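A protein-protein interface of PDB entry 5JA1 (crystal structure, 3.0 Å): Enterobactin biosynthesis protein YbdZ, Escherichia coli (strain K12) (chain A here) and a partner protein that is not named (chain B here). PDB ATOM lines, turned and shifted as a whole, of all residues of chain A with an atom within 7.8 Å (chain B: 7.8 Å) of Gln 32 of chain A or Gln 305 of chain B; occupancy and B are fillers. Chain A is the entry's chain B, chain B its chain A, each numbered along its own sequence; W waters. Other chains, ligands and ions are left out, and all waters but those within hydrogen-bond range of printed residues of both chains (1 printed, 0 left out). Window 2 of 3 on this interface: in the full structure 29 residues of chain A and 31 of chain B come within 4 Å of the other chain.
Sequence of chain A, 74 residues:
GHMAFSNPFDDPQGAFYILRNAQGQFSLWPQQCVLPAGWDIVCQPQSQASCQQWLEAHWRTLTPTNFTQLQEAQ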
ATOM      1  N   ASN A   7      11.888  12.311  23.552  1.00  0.00           N
ATOM      2  CA  ASN A   7      11.718  10.921  23.143  1.00  0.00           C
ATOM      3  C   ASN A   7      10.486  10.325  23.821  1.00  0.00           C
ATOM      4  O   ASN A   7      10.323  10.474  25.041  1.00  0.00           O
ATOM      5  CB  ASN A   7      12.970  10.123  23.503  1.00  0.00           C
ATOM      6  CG  ASN A   7      13.125   8.853  22.683  1.00  0.00           C
ATOM      7  OD1 ASN A   7      12.161   8.131  22.436  1.00  0.00           O
ATOM      8  ND2 ASN A   7      14.354   8.572  22.263  1.00  0.00           N
ATOM      9  N   PRO A   8       9.593   9.658  23.077  1.00  0.00           N
ATOM     10  CA  PRO A   8       8.392   9.086  23.711  1.00  0.00           C
ATOM     11  C   PRO A   8       8.679   7.953  24.683  1.00  0.00           C
ATOM     12  O   PRO A   8       7.787   7.599  25.464  1.00  0.00           O
ATOM     13  CB  PRO A   8       7.566   8.593  22.514  1.00  0.00           C
ATOM     14  CG  PRO A   8       8.558   8.400  21.424  1.00  0.00           C
ATOM     15  CD  PRO A   8       9.563   9.499  21.613  1.00  0.00           C
ATOM     16  N   PHE A   9       9.879   7.367  24.664  1.00  0.00           N
ATOM     17  CA  PHE A   9      10.200   6.304  25.609  1.00  0.00           C
ATOM     18  C   PHE A   9      10.691   6.834  26.947  1.00  0.00           C
ATOM     19  O   PHE A   9      10.637   6.105  27.945  1.00  0.00           O
ATOM     20  CB  PHE A   9      11.255   5.366  25.021  1.00  0.00           C
ATOM     21  CG  PHE A   9      10.705   4.364  24.048  1.00  0.00           C
ATOM     22  CD1 PHE A   9      10.246   3.134  24.487  1.00  0.00           C
ATOM     23  CD2 PHE A   9      10.656   4.649  22.695  1.00  0.00           C
ATOM     24  CE1 PHE A   9       9.745   2.209  23.593  1.00  0.00           C
ATOM     25  CE2 PHE A   9      10.155   3.728  21.797  1.00  0.00           C
ATOM     26  CZ  PHE A   9       9.702   2.508  22.245  1.00  0.00           C
ATOM     27  N   ASP A  11       9.240   9.118  28.609  1.00  0.00           N
ATOM     28  CA  ASP A  11       8.085   9.689  29.292  1.00  0.00           C
ATOM     29  C   ASP A  11       7.708   8.828  30.491  1.00  0.00           C
ATOM     30  O   ASP A  11       7.170   7.727  30.320  1.00  0.00           O
ATOM     31  CB  ASP A  11       6.904   9.819  28.328  1.00  0.00           C
ATOM     32  CG  ASP A  11       5.686  10.451  28.975  1.00  0.00           C
ATOM     33  OD1 ASP A  11       5.835  11.100  30.032  1.00  0.00           O
ATOM     34  OD2 ASP A  11       4.577  10.304  28.419  1.00  0.00           O
ATOM     35  N   GLY A  14       4.096   7.782  30.627  1.00  0.00           N
ATOM     36  CA  GLY A  14       3.572   7.103  29.462  1.00  0.00           C
ATOM     37  C   GLY A  14       3.203   5.657  29.739  1.00  0.00           C
ATOM     38  O   GLY A  14       3.735   5.007  30.637  1.00  0.00           O
ATOM     39  N   ALA A  15       2.261   5.160  28.945  1.00  0.00           N
ATOM     40  CA  ALA A  15       1.868   3.760  28.957  1.00  0.00           C
ATOM     41  C   ALA A  15       2.565   3.032  27.815  1.00  0.00           C
ATOM     42  O   ALA A  15       2.834   3.611  26.760  1.00  0.00           O
ATOM     43  CB  ALA A  15       0.351   3.612  28.830  1.00  0.00           C
ATOM     44  N   PHE A  16       2.861   1.754  28.034  1.00  0.00           N
ATOM     45  CA  PHE A  16       3.656   0.993  27.079  1.00  0.00           C
ATOM     46  C   PHE A  16       3.137  -0.429  26.958  1.00  0.00           C
ATOM     47  O   PHE A  16       2.924  -1.104  27.969  1.00  0.00           O
ATOM     48  CB  PHE A  16       5.132   0.963  27.493  1.00  0.00           C
ATOM     49  CG  PHE A  16       5.785   2.313  27.507  1.00  0.00           C
ATOM     50  CD1 PHE A  16       6.339   2.840  26.353  1.00  0.00           C
ATOM     51  CD2 PHE A  16       5.848   3.054  28.674  1.00  0.00           C
ATOM     52  CE1 PHE A  16       6.945   4.085  26.362  1.00  0.00           C
ATOM     53  CE2 PHE A  16       6.450   4.298  28.691  1.00  0.00           C
ATOM     54  CZ  PHE A  16       7.000   4.814  27.534  1.00  0.00           C
ATOM     55  N   TYR A  17       2.941  -0.879  25.719  1.00  0.00           N
ATOM     56  CA  TYR A  17       2.803  -2.301  25.459  1.00  0.00           C
ATOM     57  C   TYR A  17       4.120  -3.011  25.757  1.00  0.00           C
ATOM     58  O   TYR A  17       5.183  -2.393  25.862  1.00  0.00           O
ATOM     59  CB  TYR A  17       2.428  -2.566  24.000  1.00  0.00           C
ATOM     60  CG  TYR A  17       1.112  -1.994  23.528  1.00  0.00           C
ATOM     61  CD1 TYR A  17      -0.061  -2.734  23.619  1.00  0.00           C
ATOM     62  CD2 TYR A  17       1.047  -0.733  22.952  1.00  0.00           C
ATOM     63  CE1 TYR A  17      -1.264  -2.222  23.173  1.00  0.00           C
ATOM     64  CE2 TYR A  17      -0.153  -0.213  22.502  1.00  0.00           C
ATOM     65  CZ  TYR A  17      -1.305  -0.961  22.616  1.00  0.00           C
ATOM     66  OH  TYR A  17      -2.500  -0.445  22.169  1.00  0.00           O
ATOM     67  N   TRP A  29       6.541  -0.755  23.621  1.00  0.00           N
ATOM     68  CA  TRP A  29       6.009   0.075  22.557  1.00  0.00           C
ATOM     69  C   TRP A  29       5.046   1.089  23.162  1.00  0.00           C
ATOM     70  O   TRP A  29       4.125   0.702  23.904  1.00  0.00           O
ATOM     71  CB  TRP A  29       5.306  -0.747  21.473  1.00  0.00           C
ATOM     72  CG  TRP A  29       5.121   0.036  20.214  1.00  0.00           C
ATOM     73  CD1 TRP A  29       3.953   0.553  19.734  1.00  0.00           C
ATOM     74  CD2 TRP A  29       6.144   0.422  19.288  1.00  0.00           C
ATOM     75  NE1 TRP A  29       4.183   1.224  18.557  1.00  0.00           N
ATOM     76  CE2 TRP A  29       5.521   1.160  18.262  1.00  0.00           C
ATOM     77  CE3 TRP A  29       7.524   0.209  19.222  1.00  0.00           C
ATOM     78  CZ2 TRP A  29       6.229   1.685  17.182  1.00  0.00           C
ATOM     79  CZ3 TRP A  29       8.228   0.732  18.150  1.00  0.00           C
ATOM     80  CH2 TRP A  29       7.579   1.461  17.145  1.00  0.00           C
ATOM     81  N   PRO A  30       5.224   2.377  22.881  1.00  0.00           N
ATOM     82  CA  PRO A  30       4.336   3.388  23.462  1.00  0.00           C
ATOM     83  C   PRO A  30       2.914   3.234  22.946  1.00  0.00           C
ATOM     84  O   PRO A  30       2.686   2.957  21.766  1.00  0.00           O
ATOM     85  CB  PRO A  30       4.963   4.713  23.014  1.00  0.00           C
ATOM     86  CG  PRO A  30       5.757   4.367  21.801  1.00  0.00           C
ATOM     87  CD  PRO A  30       6.243   2.964  21.996  1.00  0.00           C
ATOM     88  N   GLN A  31       1.955   3.413  23.858  1.00  0.00           N
ATOM     89  CA  GLN A  31       0.549   3.201  23.531  1.00  0.00           C
ATOM     90  C   GLN A  31       0.093   4.080  22.373  1.00  0.00           C
ATOM     91  O   GLN A  31      -0.786   3.681  21.599  1.00  0.00           O
ATOM     92  CB  GLN A  31      -0.309   3.459  24.771  1.00  0.00           C
ATOM     93  CG  GLN A  31      -1.791   3.179  24.591  1.00  0.00           C
ATOM     94  CD  GLN A  31      -2.604   3.562  25.811  1.00  0.00           C
ATOM     95  OE1 GLN A  31      -2.114   4.258  26.701  1.00  0.00           O
ATOM     96  NE2 GLN A  31      -3.852   3.108  25.862  1.00  0.00           N
ATOM     97  N   GLN A  32       0.687   5.261  22.221  1.00  0.00           N
ATOM     98  CA  GLN A  32       0.222   6.240  21.245  1.00  0.00           C
ATOM     99  C   GLN A  32       0.731   5.982  19.833  1.00  0.00           C
ATOM    100  O   GLN A  32       0.395   6.751  18.926  1.00  0.00           O
ATOM    101  CB  GLN A  32       0.633   7.648  21.686  1.00  0.00           C
ATOM    102  CG  GLN A  32       2.136   7.889  21.737  1.00  0.00           C
ATOM    103  CD  GLN A  32       2.773   7.413  23.027  1.00  0.00           C
ATOM    104  OE1 GLN A  32       2.235   6.550  23.724  1.00  0.00           O
ATOM    105  NE2 GLN A  32       3.930   7.977  23.356  1.00  0.00           N
ATOM    106  N   CYS A  33       1.516   4.933  19.612  1.00  0.00           N
ATOM    107  CA  CYS A  33       2.112   4.675  18.310  1.00  0.00           C
ATOM    108  C   CYS A  33       1.523   3.416  17.686  1.00  0.00           C
ATOM    109  O   CYS A  33       1.117   2.484  18.388  1.00  0.00           O
ATOM    110  CB  CYS A  33       3.634   4.539  18.423  1.00  0.00           C
ATOM    111  SG  CYS A  33       4.446   6.021  19.065  1.00  0.00           S
ATOM    112  N   VAL A  34       1.480   3.404  16.355  1.00  0.00           N
ATOM    113  CA  VAL A  34       0.975   2.248  15.627  1.00  0.00           C
ATOM    114  C   VAL A  34       1.892   1.052  15.850  1.00  0.00           C
ATOM    115  O   VAL A  34       3.117   1.166  15.743  1.00  0.00           O
ATOM    116  CB  VAL A  34       0.860   2.565  14.138  1.00  0.00           C
ATOM    117  N   LEU A  35       1.294  -0.096  16.159  1.00  0.00           N
ATOM    118  CA  LEU A  35       2.073  -1.267  16.533  1.00  0.00           C
ATOM    119  C   LEU A  35       2.929  -1.742  15.360  1.00  0.00           C
ATOM    120  O   LEU A  35       2.484  -1.706  14.208  1.00  0.00           O
ATOM    121  CB  LEU A  35       1.158  -2.399  16.997  1.00  0.00           C
ATOM    122  CG  LEU A  35       0.504  -2.221  18.367  1.00  0.00           C
ATOM    123  CD1 LEU A  35      -0.390  -3.405  18.679  1.00  0.00           C
ATOM    124  CD2 LEU A  35       1.557  -2.040  19.449  1.00  0.00           C
ATOM    125  N   PRO A  45      -0.999  -2.049  27.782  1.00  0.00           N
ATOM    126  CA  PRO A  45      -0.241  -0.876  28.251  1.00  0.00           C
ATOM    127  C   PRO A  45      -0.187  -0.722  29.765  1.00  0.00           C
ATOM    128  O   PRO A  45      -1.224  -0.652  30.432  1.00  0.00           O
ATOM    129  CB  PRO A  45      -0.988   0.293  27.601  1.00  0.00           C
ATOM    130  CG  PRO A  45      -1.513  -0.281  26.335  1.00  0.00           C
ATOM    131  CD  PRO A  45      -1.892  -1.704  26.660  1.00  0.00           C
ATOM    132  N   ILE B 302       0.631  21.002  18.282  1.00  0.00           N
ATOM    133  CA  ILE B 302       0.152  19.907  17.448  1.00  0.00           C
ATOM    134  C   ILE B 302       0.080  18.664  18.323  1.00  0.00           C
ATOM    135  O   ILE B 302       1.110  18.097  18.704  1.00  0.00           O
ATOM    136  CB  ILE B 302       1.058  19.683  16.230  1.00  0.00           C
ATOM    137  CG1 ILE B 302       1.221  20.977  15.426  1.00  0.00           C
ATOM    138  CG2 ILE B 302       0.502  18.567  15.353  1.00  0.00           C
ATOM    139  CD1 ILE B 302      -0.062  21.483  14.802  1.00  0.00           C
ATOM    140  N   ALA B 303      -1.136  18.242  18.657  1.00  0.00           N
ATOM    141  CA  ALA B 303      -1.348  17.023  19.426  1.00  0.00           C
ATOM    142  C   ALA B 303      -1.378  15.833  18.473  1.00  0.00           C
ATOM    143  O   ALA B 303      -2.215  15.777  17.566  1.00  0.00           O
ATOM    144  CB  ALA B 303      -2.640  17.111  20.234  1.00  0.00           C
ATOM    145  N   ALA B 304      -0.472  14.877  18.690  1.00  0.00           N
ATOM    146  CA  ALA B 304      -0.295  13.783  17.741  1.00  0.00           C
ATOM    147  C   ALA B 304      -1.520  12.882  17.660  1.00  0.00           C
ATOM    148  O   ALA B 304      -1.796  12.311  16.598  1.00  0.00           O
ATOM    149  CB  ALA B 304       0.940  12.963  18.116  1.00  0.00           C
ATOM    150  N   GLN B 305      -2.262  12.739  18.754  1.00  0.00           N
ATOM    151  CA  GLN B 305      -3.408  11.841  18.798  1.00  0.00           C
ATOM    152  C   GLN B 305      -4.700  12.486  18.313  1.00  0.00           C
ATOM    153  O   GLN B 305      -5.732  11.810  18.272  1.00  0.00           O
ATOM    154  CB  GLN B 305      -3.611  11.314  20.221  1.00  0.00           C
ATOM    155  CG  GLN B 305      -2.584  10.291  20.669  1.00  0.00           C
ATOM    156  CD  GLN B 305      -2.890   9.731  22.044  1.00  0.00           C
ATOM    157  OE1 GLN B 305      -3.541  10.381  22.863  1.00  0.00           O
ATOM    158  NE2 GLN B 305      -2.430   8.514  22.302  1.00  0.00           N
ATOM    159  N   GLU B 306      -4.676  13.764  17.946  1.00  0.00           N
ATOM    160  CA  GLU B 306      -5.891  14.437  17.516  1.00  0.00           C
ATOM    161  C   GLU B 306      -6.176  14.176  16.041  1.00  0.00           C
ATOM    162  O   GLU B 306      -5.295  13.800  15.263  1.00  0.00           O
ATOM    163  CB  GLU B 306      -5.790  15.943  17.750  1.00  0.00           C
ATOM    164  CG  GLU B 306      -6.149  16.397  19.152  1.00  0.00           C
ATOM    165  CD  GLU B 306      -6.280  17.903  19.247  1.00  0.00           C
ATOM    166  OE1 GLU B 306      -5.900  18.592  18.275  1.00  0.00           O
ATOM    167  OE2 GLU B 306      -6.765  18.401  20.286  1.00  0.00           O
ATOM    168  N   THR B 307      -7.433  14.388  15.663  1.00  0.00           N
ATOM    169  CA  THR B 307      -7.831  14.395  14.266  1.00  0.00           C
ATOM    170  C   THR B 307      -7.781  15.820  13.721  1.00  0.00           C
ATOM    171  O   THR B 307      -7.642  16.794  14.464  1.00  0.00           O
ATOM    172  CB  THR B 307      -9.234  13.808  14.093  1.00  0.00           C
ATOM    173  OG1 THR B 307     -10.174  14.571  14.860  1.00  0.00           O
ATOM    174  CG2 THR B 307      -9.271  12.358  14.549  1.00  0.00           C
ATOM    175  N   LEU B 308      -7.888  15.934  12.399  1.00  0.00           N
ATOM    176  CA  LEU B 308      -7.887  17.255  11.777  1.00  0.00           C
ATOM    177  C   LEU B 308      -9.058  18.130  12.217  1.00  0.00           C
ATOM    178  O   LEU B 308      -8.842  19.339  12.416  1.00  0.00           O
ATOM    179  CB  LEU B 308      -7.848  17.105  10.252  1.00  0.00           C
ATOM    180  CG  LEU B 308      -7.677  18.398   9.453  1.00  0.00           C
ATOM    181  CD1 LEU B 308      -6.499  19.207   9.978  1.00  0.00           C
ATOM    182  CD2 LEU B 308      -7.513  18.098   7.972  1.00  0.00           C
ATOM    183  N   GLU B 310     -10.542  18.214  15.189  1.00  0.00           N
ATOM    184  CA  GLU B 310     -10.269  18.676  16.545  1.00  0.00           C
ATOM    185  C   GLU B 310      -9.194  19.756  16.557  1.00  0.00           C
ATOM    186  O   GLU B 310      -9.321  20.757  17.272  1.00  0.00           O
ATOM    187  CB  GLU B 310      -9.868  17.495  17.427  1.00  0.00           C
ATOM    188  CG  GLU B 310     -10.953  16.436  17.548  1.00  0.00           C
ATOM    189  CD  GLU B 310     -10.508  15.219  18.332  1.00  0.00           C
ATOM    190  OE1 GLU B 310      -9.295  15.089  18.597  1.00  0.00           O
ATOM    191  OE2 GLU B 310     -11.373  14.389  18.684  1.00  0.00           O
ATOM    192  N   ALA B 427     -10.398  10.553   9.471  1.00  0.00           N
ATOM    193  CA  ALA B 427     -10.144  10.111  10.834  1.00  0.00           C
ATOM    194  C   ALA B 427      -8.661   9.904  11.109  1.00  0.00           C
ATOM    195  O   ALA B 427      -8.306   9.344  12.151  1.00  0.00           O
ATOM    196  CB  ALA B 427     -10.911   8.820  11.126  1.00  0.00           C
ATOM    197  N   LEU B 428      -7.797  10.339  10.197  1.00  0.00           N
ATOM    198  CA  LEU B 428      -6.361  10.187  10.374  1.00  0.00           C
ATOM    199  C   LEU B 428      -5.865  11.064  11.517  1.00  0.00           C
ATOM    200  O   LEU B 428      -6.356  12.176  11.726  1.00  0.00           O
ATOM    201  CB  LEU B 428      -5.635  10.545   9.077  1.00  0.00           C
ATOM    202  CG  LEU B 428      -4.108  10.495   9.063  1.00  0.00           C
ATOM    203  CD1 LEU B 428      -3.618   9.065   9.213  1.00  0.00           C
ATOM    204  CD2 LEU B 428      -3.564  11.127   7.790  1.00  0.00           C
ATOM    205  N   LEU B 429      -4.887  10.555  12.260  1.00  0.00           N
ATOM    206  CA  LEU B 429      -4.286  11.319  13.344  1.00  0.00           C
ATOM    207  C   LEU B 429      -3.226  12.267  12.800  1.00  0.00           C
ATOM    208  O   LEU B 429      -2.515  11.944  11.842  1.00  0.00           O
ATOM    209  CB  LEU B 429      -3.667  10.387  14.386  1.00  0.00           C
ATOM    210  CG  LEU B 429      -4.585   9.352  15.036  1.00  0.00           C
ATOM    211  CD1 LEU B 429      -3.854   8.611  16.147  1.00  0.00           C
ATOM    212  CD2 LEU B 429      -5.854  10.004  15.560  1.00  0.00           C
ATOM    213  N   CYS B 430      -3.120  13.444  13.423  1.00  0.00           N
ATOM    214  CA  CYS B 430      -2.139  14.433  12.995  1.00  0.00           C
ATOM    215  C   CYS B 430      -0.705  13.964  13.222  1.00  0.00           C
ATOM    216  O   CYS B 430       0.203  14.428  12.526  1.00  0.00           O
ATOM    217  CB  CYS B 430      -2.377  15.757  13.723  1.00  0.00           C
ATOM    218  SG  CYS B 430      -3.984  16.527  13.402  1.00  0.00           S
ATOM    219  N   GLY B 431      -0.477  13.056  14.175  1.00  0.00           N
ATOM    220  CA  GLY B 431       0.860  12.543  14.409  1.00  0.00           C
ATOM    221  C   GLY B 431       1.290  11.450  13.457  1.00  0.00           C
ATOM    222  O   GLY B 431       2.493  11.208  13.310  1.00  0.00           O
ATOM    223  N   ASP B 432       0.340  10.789  12.798  1.00  0.00           N
ATOM    224  CA  ASP B 432       0.637   9.689  11.891  1.00  0.00           C
ATOM    225  C   ASP B 432       0.601  10.100  10.425  1.00  0.00           C
ATOM    226  O   ASP B 432       0.780   9.245   9.554  1.00  0.00           O
ATOM    227  CB  ASP B 432      -0.340   8.532  12.125  1.00  0.00           C
ATOM    228  CG  ASP B 432      -0.305   8.023  13.554  1.00  0.00           C
ATOM    229  OD1 ASP B 432       0.761   8.134  14.195  1.00  0.00           O
ATOM    230  OD2 ASP B 432      -1.340   7.516  14.037  1.00  0.00           O
ATOM    231  N   ALA B 791       8.689  11.543  17.063  1.00  0.00           N
ATOM    232  CA  ALA B 791       8.097  10.958  18.262  1.00  0.00           C
ATOM    233  C   ALA B 791       7.090   9.864  17.934  1.00  0.00           C
ATOM    234  O   ALA B 791       6.885   8.955  18.746  1.00  0.00           O
ATOM    235  CB  ALA B 791       7.430  12.045  19.106  1.00  0.00           C
ATOM    236  N   MET B 792       6.450   9.933  16.769  1.00  0.00           N
ATOM    237  CA  MET B 792       5.519   8.904  16.330  1.00  0.00           C
ATOM    238  C   MET B 792       6.188   7.835  15.471  1.00  0.00           C
ATOM    239  O   MET B 792       5.488   7.069  14.800  1.00  0.00           O
ATOM    240  CB  MET B 792       4.355   9.539  15.564  1.00  0.00           C
ATOM    241  CG  MET B 792       3.475  10.457  16.404  1.00  0.00           C
ATOM    242  SD  MET B 792       2.578   9.594  17.708  1.00  0.00           S
ATOM    243  CE  MET B 792       3.495  10.111  19.156  1.00  0.00           C
ATOM    244  N   MET B 793       7.524   7.780  15.478  1.00  0.00           N
ATOM    245  CA  MET B 793       8.303   6.754  14.784  1.00  0.00           C
ATOM    246  C   MET B 793       8.160   6.838  13.265  1.00  0.00           C
ATOM    247  O   MET B 793       8.170   5.816  12.577  1.00  0.00           O
ATOM    248  CB  MET B 793       7.942   5.349  15.278  1.00  0.00           C
ATOM    249  CG  MET B 793       8.052   5.194  16.786  1.00  0.00           C
ATOM    250  SD  MET B 793       9.725   5.504  17.378  1.00  0.00           S
ATOM    251  CE  MET B 793       9.424   5.777  19.121  1.00  0.00           C
ATOM    252  N   HIS B 794       8.036   8.056  12.733  1.00  0.00           N
ATOM    253  CA  HIS B 794       8.001   8.324  11.305  1.00  0.00           C
ATOM    254  C   HIS B 794       9.278   9.038  10.871  1.00  0.00           C
ATOM    255  O   HIS B 794       9.845   9.821  11.638  1.00  0.00           O
ATOM    256  CB  HIS B 794       6.788   9.185  10.928  1.00  0.00           C
ATOM    257  CG  HIS B 794       5.471   8.533  11.216  1.00  0.00           C
ATOM    258  ND1 HIS B 794       5.054   7.384  10.579  1.00  0.00           N
ATOM    259  CD2 HIS B 794       4.475   8.873  12.069  1.00  0.00           C
ATOM    260  CE1 HIS B 794       3.860   7.042  11.030  1.00  0.00           C
ATOM    261  NE2 HIS B 794       3.486   7.929  11.934  1.00  0.00           N
HETATM  262  O   HOH W   1       2.717   6.059  15.246  1.00  0.00           O
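Water W1 lies within hydrogen-bond range of O of Met 792 of chain B (3.0 Å), OD1 of Asp 432 of chain B (3.0 Å) and N of Val 34 of chain A (3.1 Å).
The side-chain amide oxygen (OD1) of Asn 7 of chain A sits close to the backbone NH (N) of Phe 9 of chain A. The backbone NH (N) of Tyr 17 of chain A lies within hydrogen-bond range of the backbone carbonyl oxygen (O) of Trp 29 of chain A (2.7 Å). The backbone carbonyl oxygen of Cys 33 of chain A sits at hydrogen-bond distance from the indole nitrogen of Trp 29 of chain A (3.3 Å). NE1 of Trp 29 of chain A is in hydrogen-bond range of O of Val 34 of chain A (3.0 Å).
Printed residues of chain B that touch a printed residue of chain A: Gln 305, Ala 791, Met 792 and Met 793. Of the 16 printed residues of chain A, 5 touch a printed residue of chain B. Printed residues of chain A that touch a printed residue of chain B: Pro 8, Phe 9, Trp 29, Gln 32 and Cys 33. Among the printed residues, 7 pairs touch across the chains. Among the printed residues, no Asp or Glu carboxylate lies within 4 Å of a Lys or Arg side-chain nitrogen of the other chain.
Ala 791 of chain B touches Pro 8 of chain A (O to CG, 3.2 Å). CG of Pro 8 of chain A touches CE of Met 793 of chain B, at 3.6 Å. Met 793 of chain B touches Phe 9 of chain A (CE to CE2, 3.4 Å). CH2 of Trp 29 of chain A touches CG of Met 793 of chain B, at 3.8 Å. Gln 32 of chain A touches Gln 305 of chain B. Ala 791 of chain B touches Cys 33 of chain A.
Of the printed residues of chain B, Trp 29 of chain A touches Met 793 (3.8 Å). Of chain B, only Gln 305 (3.2 Å) and Met 792 (3.7 Å) come within 4 Å of Gln 32 of chain A. No residue of chain A comes within 4 Å of Ala 304 of chain B. Gln 305 of chain B touches just one residue of chain A: Gln 32. Thr 307 of chain B touches none of the printed residues of chain A. Printed residues of chain A within 4 Å of Met 792 of chain B: Gln 32 (3.7 Å). The nearest residue of chain B that does not touch Gln 32 of chain A is Asp 432 of chain B (4.9 Å). The nearest printed residue of chain A that does not touch Met 793 of chain B is Cys 33 of chain A (4.3 Å).
O of Gln 32 of chain A lies close to SD of Met 792 of chain B, at 3.8 Å.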
